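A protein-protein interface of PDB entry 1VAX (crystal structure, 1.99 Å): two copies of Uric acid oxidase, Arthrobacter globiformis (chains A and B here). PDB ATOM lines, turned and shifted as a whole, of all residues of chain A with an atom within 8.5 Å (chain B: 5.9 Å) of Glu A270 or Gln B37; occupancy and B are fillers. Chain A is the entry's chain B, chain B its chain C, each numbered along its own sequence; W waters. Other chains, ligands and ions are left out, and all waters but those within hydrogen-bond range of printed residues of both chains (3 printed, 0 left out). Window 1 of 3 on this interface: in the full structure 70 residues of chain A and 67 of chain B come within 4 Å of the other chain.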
ATOM      1  N   SER A 177      30.988  19.331   9.495  1.00  0.00           N
ATOM      2  CA  SER A 177      30.651  18.907  10.843  1.00  0.00           C
ATOM      3  C   SER A 177      31.612  17.764  11.130  1.00  0.00           C
ATOM      4  O   SER A 177      31.576  16.728  10.463  1.00  0.00           O
ATOM      5  CB  SER A 177      29.212  18.407  10.931  1.00  0.00           C
ATOM      6  OG  SER A 177      28.312  19.492  11.046  1.00  0.00           O
ATOM      7  N   LEU A 212      31.961  12.774  -2.730  1.00  0.00           N
ATOM      8  CA  LEU A 212      32.014  13.445  -1.431  1.00  0.00           C
ATOM      9  C   LEU A 212      32.665  12.481  -0.440  1.00  0.00           C
ATOM     10  O   LEU A 212      33.375  12.903   0.483  1.00  0.00           O
ATOM     11  CB  LEU A 212      30.605  13.801  -0.946  1.00  0.00           C
ATOM     12  CG  LEU A 212      30.419  15.059  -0.088  1.00  0.00           C
ATOM     13  CD1 LEU A 212      29.070  14.992   0.587  1.00  0.00           C
ATOM     14  CD2 LEU A 212      31.517  15.190   0.945  1.00  0.00           C
ATOM     15  N   GLN A 213      32.417  11.185  -0.640  1.00  0.00           N
ATOM     16  CA  GLN A 213      32.979  10.146   0.223  1.00  0.00           C
ATOM     17  C   GLN A 213      34.503  10.178   0.223  1.00  0.00           C
ATOM     18  O   GLN A 213      35.134   9.982   1.263  1.00  0.00           O
ATOM     19  CB  GLN A 213      32.501   8.752  -0.208  1.00  0.00           C
ATOM     20  CG  GLN A 213      31.045   8.441   0.145  1.00  0.00           C
ATOM     21  CD  GLN A 213      30.068   8.781  -0.971  1.00  0.00           C
ATOM     22  OE1 GLN A 213      30.280   9.725  -1.726  1.00  0.00           O
ATOM     23  NE2 GLN A 213      28.981   8.019  -1.063  1.00  0.00           N
ATOM     24  N   MET A 216      35.789  13.402   1.996  1.00  0.00           N
ATOM     25  CA  MET A 216      35.649  13.210   3.428  1.00  0.00           C
ATOM     26  C   MET A 216      36.742  12.279   3.945  1.00  0.00           C
ATOM     27  O   MET A 216      37.330  12.525   5.000  1.00  0.00           O
ATOM     28  CB  MET A 216      34.270  12.635   3.757  1.00  0.00           C
ATOM     29  CG  MET A 216      34.073  12.323   5.235  1.00  0.00           C
ATOM     30  SD  MET A 216      32.382  11.851   5.607  1.00  0.00           S
ATOM     31  CE  MET A 216      32.286  10.319   4.644  1.00  0.00           C
ATOM     32  N   TYR A 217      37.020  11.212   3.202  1.00  0.00           N
ATOM     33  CA  TYR A 217      38.058  10.276   3.619  1.00  0.00           C
ATOM     34  C   TYR A 217      39.393  11.000   3.731  1.00  0.00           C
ATOM     35  O   TYR A 217      40.113  10.849   4.719  1.00  0.00           O
ATOM     36  CB  TYR A 217      38.201   9.126   2.615  1.00  0.00           C
ATOM     37  CG  TYR A 217      39.270   8.131   3.011  1.00  0.00           C
ATOM     38  CD1 TYR A 217      39.038   7.195   4.017  1.00  0.00           C
ATOM     39  CD2 TYR A 217      40.523   8.144   2.398  1.00  0.00           C
ATOM     40  CE1 TYR A 217      40.030   6.291   4.406  1.00  0.00           C
ATOM     41  CE2 TYR A 217      41.521   7.246   2.779  1.00  0.00           C
ATOM     42  CZ  TYR A 217      41.267   6.324   3.782  1.00  0.00           C
ATOM     43  OH  TYR A 217      42.247   5.431   4.161  1.00  0.00           O
ATOM     44  N   ILE A 233      38.024  10.245  14.027  1.00  0.00           N
ATOM     45  CA  ILE A 233      37.288  11.448  13.696  1.00  0.00           C
ATOM     46  C   ILE A 233      36.077  11.032  12.881  1.00  0.00           C
ATOM     47  O   ILE A 233      36.180  10.223  11.946  1.00  0.00           O
ATOM     48  CB  ILE A 233      38.157  12.459  12.901  1.00  0.00           C
ATOM     49  CG1 ILE A 233      37.330  13.706  12.560  1.00  0.00           C
ATOM     50  CG2 ILE A 233      38.701  11.806  11.636  1.00  0.00           C
ATOM     51  CD1 ILE A 233      38.156  14.863  11.992  1.00  0.00           C
ATOM     52  N   LYS A 234      34.926  11.558  13.282  1.00  0.00           N
ATOM     53  CA  LYS A 234      33.662  11.285  12.629  1.00  0.00           C
ATOM     54  C   LYS A 234      33.191  12.546  11.931  1.00  0.00           C
ATOM     55  O   LYS A 234      33.234  13.639  12.497  1.00  0.00           O
ATOM     56  CB  LYS A 234      32.609  10.862  13.657  1.00  0.00           C
ATOM     57  CG  LYS A 234      32.955   9.594  14.415  1.00  0.00           C
ATOM     58  CD  LYS A 234      31.731   9.049  15.132  1.00  0.00           C
ATOM     59  CE  LYS A 234      32.006   7.671  15.709  1.00  0.00           C
ATOM     60  NZ  LYS A 234      30.768   7.089  16.292  1.00  0.00           N
ATOM     61  N   MET A 235      32.731  12.393  10.699  1.00  0.00           N
ATOM     62  CA  MET A 235      32.254  13.539   9.952  1.00  0.00           C
ATOM     63  C   MET A 235      30.884  13.277   9.355  1.00  0.00           C
ATOM     64  O   MET A 235      30.557  12.144   9.000  1.00  0.00           O
ATOM     65  CB  MET A 235      33.254  13.887   8.857  1.00  0.00           C
ATOM     66  CG  MET A 235      34.569  14.413   9.399  1.00  0.00           C
ATOM     67  SD  MET A 235      35.881  14.349   8.182  1.00  0.00           S
ATOM     68  CE  MET A 235      36.211  12.593   8.172  1.00  0.00           C
ATOM     69  N   SER A 236      30.078  14.333   9.277  1.00  0.00           N
ATOM     70  CA  SER A 236      28.742  14.257   8.707  1.00  0.00           C
ATOM     71  C   SER A 236      28.684  15.411   7.727  1.00  0.00           C
ATOM     72  O   SER A 236      28.601  16.578   8.127  1.00  0.00           O
ATOM     73  CB  SER A 236      27.675  14.432   9.785  1.00  0.00           C
ATOM     74  OG  SER A 236      26.380  14.384   9.210  1.00  0.00           O
ATOM     75  N   LEU A 237      28.736  15.083   6.441  1.00  0.00           N
ATOM     76  CA  LEU A 237      28.747  16.104   5.410  1.00  0.00           C
ATOM     77  C   LEU A 237      27.578  16.067   4.449  1.00  0.00           C
ATOM     78  O   LEU A 237      27.363  15.083   3.742  1.00  0.00           O
ATOM     79  CB  LEU A 237      30.050  16.009   4.607  1.00  0.00           C
ATOM     80  CG  LEU A 237      31.359  16.057   5.410  1.00  0.00           C
ATOM     81  CD1 LEU A 237      32.549  15.919   4.464  1.00  0.00           C
ATOM     82  CD2 LEU A 237      31.441  17.365   6.184  1.00  0.00           C
ATOM     83  N   PRO A 238      26.792  17.147   4.425  1.00  0.00           N
ATOM     84  CA  PRO A 238      25.644  17.227   3.528  1.00  0.00           C
ATOM     85  C   PRO A 238      26.128  17.669   2.151  1.00  0.00           C
ATOM     86  O   PRO A 238      27.078  18.442   2.038  1.00  0.00           O
ATOM     87  CB  PRO A 238      24.767  18.283   4.191  1.00  0.00           C
ATOM     88  CG  PRO A 238      25.778  19.210   4.797  1.00  0.00           C
ATOM     89  CD  PRO A 238      26.754  18.237   5.421  1.00  0.00           C
ATOM     90  N   TYR A 266      18.925  16.912   0.424  1.00  0.00           N
ATOM     91  CA  TYR A 266      20.362  17.049   0.264  1.00  0.00           C
ATOM     92  C   TYR A 266      21.003  15.703   0.550  1.00  0.00           C
ATOM     93  O   TYR A 266      20.471  14.909   1.323  1.00  0.00           O
ATOM     94  CB  TYR A 266      20.933  18.097   1.226  1.00  0.00           C
ATOM     95  CG  TYR A 266      20.506  17.923   2.662  1.00  0.00           C
ATOM     96  CD1 TYR A 266      19.295  18.449   3.116  1.00  0.00           C
ATOM     97  CD2 TYR A 266      21.308  17.228   3.572  1.00  0.00           C
ATOM     98  CE1 TYR A 266      18.890  18.288   4.444  1.00  0.00           C
ATOM     99  CE2 TYR A 266      20.916  17.060   4.900  1.00  0.00           C
ATOM    100  CZ  TYR A 266      19.706  17.593   5.330  1.00  0.00           C
ATOM    101  OH  TYR A 266      19.310  17.433   6.640  1.00  0.00           O
ATOM    102  N   GLY A 267      22.133  15.444  -0.093  1.00  0.00           N
ATOM    103  CA  GLY A 267      22.828  14.197   0.152  1.00  0.00           C
ATOM    104  C   GLY A 267      23.427  14.311   1.541  1.00  0.00           C
ATOM    105  O   GLY A 267      23.719  15.415   2.005  1.00  0.00           O
ATOM    106  N   LEU A 268      23.594  13.184   2.220  1.00  0.00           N
ATOM    107  CA  LEU A 268      24.176  13.199   3.557  1.00  0.00           C
ATOM    108  C   LEU A 268      25.168  12.050   3.621  1.00  0.00           C
ATOM    109  O   LEU A 268      24.777  10.885   3.696  1.00  0.00           O
ATOM    110  CB  LEU A 268      23.096  13.029   4.629  1.00  0.00           C
ATOM    111  CG  LEU A 268      23.567  13.175   6.080  1.00  0.00           C
ATOM    112  CD1 LEU A 268      24.283  14.509   6.264  1.00  0.00           C
ATOM    113  CD2 LEU A 268      22.370  13.080   7.019  1.00  0.00           C
ATOM    114  N   ILE A 269      26.449  12.401   3.562  1.00  0.00           N
ATOM    115  CA  ILE A 269      27.550  11.444   3.593  1.00  0.00           C
ATOM    116  C   ILE A 269      28.193  11.511   4.972  1.00  0.00           C
ATOM    117  O   ILE A 269      28.606  12.580   5.412  1.00  0.00           O
ATOM    118  CB  ILE A 269      28.590  11.796   2.496  1.00  0.00           C
ATOM    119  CG1 ILE A 269      28.102  11.305   1.134  1.00  0.00           C
ATOM    120  CG2 ILE A 269      29.926  11.160   2.799  1.00  0.00           C
ATOM    121  CD1 ILE A 269      26.751  11.837   0.718  1.00  0.00           C
ATOM    122  N   GLU A 270      28.267  10.371   5.655  1.00  0.00           N
ATOM    123  CA  GLU A 270      28.839  10.327   6.998  1.00  0.00           C
ATOM    124  C   GLU A 270      29.820   9.168   7.137  1.00  0.00           C
ATOM    125  O   GLU A 270      29.608   8.098   6.561  1.00  0.00           O
ATOM    126  CB  GLU A 270      27.705  10.189   8.023  1.00  0.00           C
ATOM    127  CG  GLU A 270      26.514  11.119   7.725  1.00  0.00           C
ATOM    128  CD  GLU A 270      25.469  11.149   8.828  1.00  0.00           C
ATOM    129  OE1 GLU A 270      25.606  11.978   9.752  1.00  0.00           O
ATOM    130  OE2 GLU A 270      24.513  10.342   8.776  1.00  0.00           O
ATOM    131  N   ALA A 271      30.893   9.376   7.899  1.00  0.00           N
ATOM    132  CA  ALA A 271      31.884   8.321   8.085  1.00  0.00           C
ATOM    133  C   ALA A 271      32.808   8.550   9.261  1.00  0.00           C
ATOM    134  O   ALA A 271      33.007   9.677   9.714  1.00  0.00           O
ATOM    135  CB  ALA A 271      32.717   8.148   6.819  1.00  0.00           C
ATOM    136  N   THR A 272      33.367   7.449   9.747  1.00  0.00           N
ATOM    137  CA  THR A 272      34.302   7.471  10.854  1.00  0.00           C
ATOM    138  C   THR A 272      35.648   7.069  10.277  1.00  0.00           C
ATOM    139  O   THR A 272      35.769   6.024   9.632  1.00  0.00           O
ATOM    140  CB  THR A 272      33.938   6.444  11.946  1.00  0.00           C
ATOM    141  OG1 THR A 272      32.625   6.712  12.452  1.00  0.00           O
ATOM    142  CG2 THR A 272      34.953   6.508  13.093  1.00  0.00           C
ATOM    143  N   ILE A 273      36.649   7.911  10.490  1.00  0.00           N
ATOM    144  CA  ILE A 273      37.992   7.632  10.022  1.00  0.00           C
ATOM    145  C   ILE A 273      38.785   7.420  11.298  1.00  0.00           C
ATOM    146  O   ILE A 273      38.810   8.287  12.179  1.00  0.00           O
ATOM    147  CB  ILE A 273      38.565   8.816   9.231  1.00  0.00           C
ATOM    148  CG1 ILE A 273      37.593   9.206   8.111  1.00  0.00           C
ATOM    149  CG2 ILE A 273      39.938   8.453   8.670  1.00  0.00           C
ATOM    150  CD1 ILE A 273      37.116   8.039   7.265  1.00  0.00           C
ATOM    151  N   GLN B   7      32.913   2.885  10.581  1.00  0.00           N
ATOM    152  CA  GLN B   7      31.487   2.883  10.287  1.00  0.00           C
ATOM    153  C   GLN B   7      31.176   4.026   9.328  1.00  0.00           C
ATOM    154  O   GLN B   7      31.789   5.091   9.398  1.00  0.00           O
ATOM    155  CB  GLN B   7      30.685   3.038  11.584  1.00  0.00           C
ATOM    156  CG  GLN B   7      30.950   1.918  12.591  1.00  0.00           C
ATOM    157  CD  GLN B   7      30.277   2.149  13.933  1.00  0.00           C
ATOM    158  OE1 GLN B   7      30.511   3.165  14.595  1.00  0.00           O
ATOM    159  NE2 GLN B   7      29.441   1.200  14.345  1.00  0.00           N
ATOM    160  N   ASN B   8      30.243   3.797   8.413  1.00  0.00           N
ATOM    161  CA  ASN B   8      29.878   4.834   7.458  1.00  0.00           C
ATOM    162  C   ASN B   8      28.521   4.556   6.842  1.00  0.00           C
ATOM    163  O   ASN B   8      28.038   3.421   6.848  1.00  0.00           O
ATOM    164  CB  ASN B   8      30.948   4.954   6.363  1.00  0.00           C
ATOM    165  CG  ASN B   8      31.081   3.690   5.517  1.00  0.00           C
ATOM    166  OD1 ASN B   8      30.326   3.476   4.568  1.00  0.00           O
ATOM    167  ND2 ASN B   8      32.041   2.846   5.870  1.00  0.00           N
ATOM    168  N   GLN B   9      27.897   5.611   6.333  1.00  0.00           N
ATOM    169  CA  GLN B   9      26.592   5.502   5.694  1.00  0.00           C
ATOM    170  C   GLN B   9      26.380   6.755   4.860  1.00  0.00           C
ATOM    171  O   GLN B   9      27.024   7.779   5.092  1.00  0.00           O
ATOM    172  CB  GLN B   9      25.481   5.372   6.742  1.00  0.00           C
ATOM    173  CG  GLN B   9      25.434   6.512   7.764  1.00  0.00           C
ATOM    174  CD  GLN B   9      24.327   6.340   8.788  1.00  0.00           C
ATOM    175  OE1 GLN B   9      23.939   5.220   9.115  1.00  0.00           O
ATOM    176  NE2 GLN B   9      23.827   7.451   9.315  1.00  0.00           N
ATOM    177  N   TYR B  10      25.489   6.676   3.881  1.00  0.00           N
ATOM    178  CA  TYR B  10      25.228   7.831   3.031  1.00  0.00           C
ATOM    179  C   TYR B  10      23.900   7.630   2.324  1.00  0.00           C
ATOM    180  O   TYR B  10      23.464   6.498   2.112  1.00  0.00           O
ATOM    181  CB  TYR B  10      26.320   7.977   1.967  1.00  0.00           C
ATOM    182  CG  TYR B  10      26.072   7.077   0.773  1.00  0.00           C
ATOM    183  CD1 TYR B  10      26.241   5.700   0.872  1.00  0.00           C
ATOM    184  CD2 TYR B  10      25.565   7.594  -0.419  1.00  0.00           C
ATOM    185  CE1 TYR B  10      25.903   4.855  -0.179  1.00  0.00           C
ATOM    186  CE2 TYR B  10      25.220   6.755  -1.481  1.00  0.00           C
ATOM    187  CZ  TYR B  10      25.391   5.386  -1.350  1.00  0.00           C
ATOM    188  OH  TYR B  10      25.036   4.544  -2.380  1.00  0.00           O
ATOM    189  N   GLY B  11      23.279   8.734   1.927  1.00  0.00           N
ATOM    190  CA  GLY B  11      22.014   8.654   1.223  1.00  0.00           C
ATOM    191  C   GLY B  11      21.407  10.029   1.052  1.00  0.00           C
ATOM    192  O   GLY B  11      22.112  11.039   1.143  1.00  0.00           O
ATOM    193  N   LYS B  12      20.103  10.079   0.794  1.00  0.00           N
ATOM    194  CA  LYS B  12      19.436  11.355   0.628  1.00  0.00           C
ATOM    195  C   LYS B  12      18.630  11.659   1.882  1.00  0.00           C
ATOM    196  O   LYS B  12      17.865  10.820   2.367  1.00  0.00           O
ATOM    197  CB  LYS B  12      18.504  11.340  -0.590  1.00  0.00           C
ATOM    198  CG  LYS B  12      17.938  12.714  -0.912  1.00  0.00           C
ATOM    199  CD  LYS B  12      18.964  13.592  -1.626  1.00  0.00           C
ATOM    200  CE  LYS B  12      19.041  13.229  -3.102  1.00  0.00           C
ATOM    201  NZ  LYS B  12      20.092  13.990  -3.826  1.00  0.00           N
ATOM    202  N   THR B  35      14.224  10.261   4.969  1.00  0.00           N
ATOM    203  CA  THR B  35      15.677  10.198   4.844  1.00  0.00           C
ATOM    204  C   THR B  35      16.069   8.735   4.594  1.00  0.00           C
ATOM    205  O   THR B  35      15.571   7.822   5.259  1.00  0.00           O
ATOM    206  CB  THR B  35      16.387  10.714   6.121  1.00  0.00           C
ATOM    207  OG1 THR B  35      16.145  12.119   6.269  1.00  0.00           O
ATOM    208  CG2 THR B  35      17.901  10.477   6.034  1.00  0.00           C
ATOM    209  N   SER B  36      16.937   8.518   3.612  1.00  0.00           N
ATOM    210  CA  SER B  36      17.397   7.173   3.268  1.00  0.00           C
ATOM    211  C   SER B  36      18.917   7.116   3.283  1.00  0.00           C
ATOM    212  O   SER B  36      19.575   7.900   2.605  1.00  0.00           O
ATOM    213  CB  SER B  36      16.892   6.779   1.874  1.00  0.00           C
ATOM    214  OG  SER B  36      17.510   5.580   1.417  1.00  0.00           O
ATOM    215  N   GLN B  37      19.476   6.196   4.065  1.00  0.00           N
ATOM    216  CA  GLN B  37      20.925   6.046   4.133  1.00  0.00           C
ATOM    217  C   GLN B  37      21.312   4.575   4.056  1.00  0.00           C
ATOM    218  O   GLN B  37      20.719   3.727   4.730  1.00  0.00           O
ATOM    219  CB  GLN B  37      21.482   6.690   5.403  1.00  0.00           C
ATOM    220  CG  GLN B  37      21.738   8.192   5.246  1.00  0.00           C
ATOM    221  CD  GLN B  37      22.318   8.817   6.491  1.00  0.00           C
ATOM    222  OE1 GLN B  37      23.182   9.691   6.417  1.00  0.00           O
ATOM    223  NE2 GLN B  37      21.845   8.376   7.645  1.00  0.00           N
ATOM    224  N   LEU B  38      22.311   4.284   3.231  1.00  0.00           N
ATOM    225  CA  LEU B  38      22.751   2.913   3.021  1.00  0.00           C
ATOM    226  C   LEU B  38      24.062   2.569   3.711  1.00  0.00           C
ATOM    227  O   LEU B  38      24.925   3.429   3.908  1.00  0.00           O
ATOM    228  CB  LEU B  38      22.898   2.637   1.520  1.00  0.00           C
ATOM    229  CG  LEU B  38      21.769   3.102   0.602  1.00  0.00           C
ATOM    230  CD1 LEU B  38      22.097   2.688  -0.830  1.00  0.00           C
ATOM    231  CD2 LEU B  38      20.437   2.506   1.040  1.00  0.00           C
ATOM    232  N   ARG B  39      24.195   1.295   4.064  1.00  0.00           N
ATOM    233  CA  ARG B  39      25.391   0.779   4.714  1.00  0.00           C
ATOM    234  C   ARG B  39      25.807  -0.496   3.986  1.00  0.00           C
ATOM    235  O   ARG B  39      24.962  -1.258   3.526  1.00  0.00           O
ATOM    236  CB  ARG B  39      25.104   0.468   6.185  1.00  0.00           C
ATOM    237  CG  ARG B  39      24.718   1.691   7.007  1.00  0.00           C
ATOM    238  CD  ARG B  39      24.131   1.287   8.353  1.00  0.00           C
ATOM    239  NE  ARG B  39      23.848   2.447   9.195  1.00  0.00           N
ATOM    240  CZ  ARG B  39      23.172   2.395  10.337  1.00  0.00           C
ATOM    241  NH1 ARG B  39      22.702   1.239  10.778  1.00  0.00           N
ATOM    242  NH2 ARG B  39      22.973   3.501  11.038  1.00  0.00           N
ATOM    243  N   HIS B  46      35.299   5.474  -0.757  1.00  0.00           N
ATOM    244  CA  HIS B  46      36.017   6.373   0.141  1.00  0.00           C
ATOM    245  C   HIS B  46      37.518   6.473  -0.123  1.00  0.00           C
ATOM    246  O   HIS B  46      38.073   7.568  -0.142  1.00  0.00           O
ATOM    247  CB  HIS B  46      35.811   5.958   1.602  1.00  0.00           C
ATOM    248  CG  HIS B  46      34.421   6.175   2.111  1.00  0.00           C
ATOM    249  ND1 HIS B  46      33.360   5.370   1.754  1.00  0.00           N
ATOM    250  CD2 HIS B  46      33.917   7.109   2.954  1.00  0.00           C
ATOM    251  CE1 HIS B  46      32.265   5.797   2.357  1.00  0.00           C
ATOM    252  NE2 HIS B  46      32.575   6.851   3.090  1.00  0.00           N
ATOM    253  N   GLN B  60      18.206   7.270  -4.796  1.00  0.00           N
ATOM    254  CA  GLN B  60      17.486   6.901  -3.581  1.00  0.00           C
ATOM    255  C   GLN B  60      16.255   7.795  -3.461  1.00  0.00           C
ATOM    256  O   GLN B  60      15.179   7.341  -3.076  1.00  0.00           O
ATOM    257  CB  GLN B  60      18.399   7.053  -2.359  1.00  0.00           C
ATOM    258  CG  GLN B  60      19.551   6.048  -2.357  1.00  0.00           C
ATOM    259  CD  GLN B  60      20.461   6.193  -1.156  1.00  0.00           C
ATOM    260  OE1 GLN B  60      20.001   6.256  -0.019  1.00  0.00           O
ATOM    261  NE2 GLN B  60      21.764   6.235  -1.404  1.00  0.00           N
ATOM    262  N   GLY B  95      22.719  -3.190   4.643  1.00  0.00           N
ATOM    263  CA  GLY B  95      21.802  -2.626   5.612  1.00  0.00           C
ATOM    264  C   GLY B  95      21.631  -1.144   5.393  1.00  0.00           C
ATOM    265  O   GLY B  95      21.948  -0.630   4.321  1.00  0.00           O
ATOM    266  N   GLY B  96      21.133  -0.455   6.412  1.00  0.00           N
ATOM    267  CA  GLY B  96      20.937   0.972   6.298  1.00  0.00           C
ATOM    268  C   GLY B  96      20.037   1.518   7.389  1.00  0.00           C
ATOM    269  O   GLY B  96      19.695   0.823   8.352  1.00  0.00           O
ATOM    270  N   ARG B  97      19.642   2.771   7.214  1.00  0.00           N
ATOM    271  CA  ARG B  97      18.792   3.464   8.162  1.00  0.00           C
ATOM    272  C   ARG B  97      17.836   4.331   7.351  1.00  0.00           C
ATOM    273  O   ARG B  97      18.263   5.176   6.565  1.00  0.00           O
ATOM    274  CB  ARG B  97      19.649   4.341   9.080  1.00  0.00           C
ATOM    275  CG  ARG B  97      18.884   5.010  10.212  1.00  0.00           C
ATOM    276  CD  ARG B  97      19.769   6.008  10.935  1.00  0.00           C
ATOM    277  NE  ARG B  97      19.065   6.694  12.017  1.00  0.00           N
ATOM    278  CZ  ARG B  97      18.919   6.211  13.250  1.00  0.00           C
ATOM    279  NH1 ARG B  97      19.432   5.029  13.579  1.00  0.00           N
ATOM    280  NH2 ARG B  97      18.256   6.916  14.160  1.00  0.00           N
ATOM    281  N   TRP B  98      16.545   4.094   7.528  1.00  0.00           N
ATOM    282  CA  TRP B  98      15.519   4.843   6.819  1.00  0.00           C
ATOM    283  C   TRP B  98      14.624   5.466   7.871  1.00  0.00           C
ATOM    284  O   TRP B  98      14.082   4.770   8.734  1.00  0.00           O
ATOM    285  CB  TRP B  98      14.735   3.898   5.906  1.00  0.00           C
ATOM    286  CG  TRP B  98      15.600   3.359   4.813  1.00  0.00           C
ATOM    287  CD1 TRP B  98      15.828   3.929   3.592  1.00  0.00           C
ATOM    288  CD2 TRP B  98      16.428   2.190   4.870  1.00  0.00           C
ATOM    289  NE1 TRP B  98      16.746   3.190   2.887  1.00  0.00           N
ATOM    290  CE2 TRP B  98      17.132   2.117   3.646  1.00  0.00           C
ATOM    291  CE3 TRP B  98      16.647   1.200   5.837  1.00  0.00           C
ATOM    292  CZ2 TRP B  98      18.041   1.086   3.360  1.00  0.00           C
ATOM    293  CZ3 TRP B  98      17.554   0.174   5.554  1.00  0.00           C
ATOM    294  CH2 TRP B  98      18.238   0.128   4.325  1.00  0.00           C
HETATM  295  O   HOH W   1      30.182   7.289  11.452  1.00  0.00           O
HETATM  296  O   HOH W   2      21.455  10.670   9.683  1.00  0.00           O
HETATM  297  O   HOH W   3      30.103   7.947   3.729  1.00  0.00           O
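O of Leu A268 lies close to OE1 of Gln B37, at 3.4 Å. The backbone carbonyl oxygen of Gly B11 is in hydrogen-bond range of the backbone NH of Leu A268 (2.8 Å). The backbone NH (N) of Glu A270 is in hydrogen-bond range of the backbone carbonyl oxygen (O) of Gln B9 (2.9 Å). The backbone carbonyl oxygen of Gln B7 sits at hydrogen-bond distance from the backbone NH of Thr A272, at 2.9 Å. OE2 of Glu A270 sits close to OE1 of Gln B37, at 2.8 Å.
The backbone NH (N) of Leu B38 is in hydrogen-bond range of the backbone carbonyl oxygen (O) of Tyr B10, at 2.7 Å. The side-chain sulfur (SD) of Met A216 lies close to the backbone NH (N) of Ala A271 (3.7 Å). The backbone carbonyl oxygen (O) of Lys B12 lies within hydrogen-bond range of the backbone NH (N) of Ser B36, 2.8 Å away. OE1 of Gln B9 is in hydrogen-bond range of NH2 of Arg B39. The backbone carbonyl oxygen of Gln B37 sits at hydrogen-bond distance from the backbone NH of Arg B97, 2.9 Å away. The backbone NH (N) of Met A235 sits at hydrogen-bond distance from the backbone carbonyl oxygen (O) of Ala A271.
Gln A213 touches Tyr B10. His B46 touches Gln A213 (CD2 to O, 3.5 Å). CE of Met A216 touches NE2 of His B46, 3.8 Å away. O of His B46 touches CB of Tyr A217, 3.2 Å away. Tyr A266 touches Lys B12 (O to CD, 3.6 Å). CA of Gly A267 touches O of Gly B11, 3.4 Å away. Lys B12 touches Gly A267 (CD to N, 3.98 Å). Leu A268 touches Tyr B10 (O to CA, 3.2 Å). C of Ile A269 touches O of Gln B9, 3.9 Å away. NE2 of His B46 touches CB of Ala A271 (3.95 Å).
Gln B37 touches two residues of chain A. Gln B9 touches just these residues of chain A: Ile A269 and Glu A270. No residue of chain A comes within 4 Å of Ser B36. Of the printed residues of chain B, Tyr A217 touches His B46. Printed residues of chain A within 4 Å of Tyr B10: Gln A213, Leu A268 and Ile A269. Gln B60 touches none of the printed residues of chain A. The nearest residue of chain A that does not touch Gln B37 is Ile A269 (5.1 Å).
Of the 17 printed residues of chain B, 8 touch a printed residue of chain A. Hydrophobic or aromatic side chains of chain B within 4 Å of the printed part of chain A: Tyr B10 and His B46. Among the printed residues, no Asp or Glu carboxylate lies within 4 Å of a Lys or Arg side-chain nitrogen of the other chain.
No position is printed for both chains. Of the 19 pairs that touch across the chains among the printed residues, none has its exchanged pair printed and touching as well.
Water W1 bridges OG1 of Thr A272 (2.7 Å) and O of Gln B7 (3.4 Å). Water W3 lies within hydrogen-bond range of a ring nitrogen (NE2) of His B46 (2.8 Å), the backbone carbonyl oxygen (O) of Glu A270 (2.9 Å) and the backbone carbonyl oxygen (O) of Gln B9 (3.4 Å). Water W2 bridges NE2 of Gln B37 (3.1 Å) and OE2 of Glu A270 (3.2 Å).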
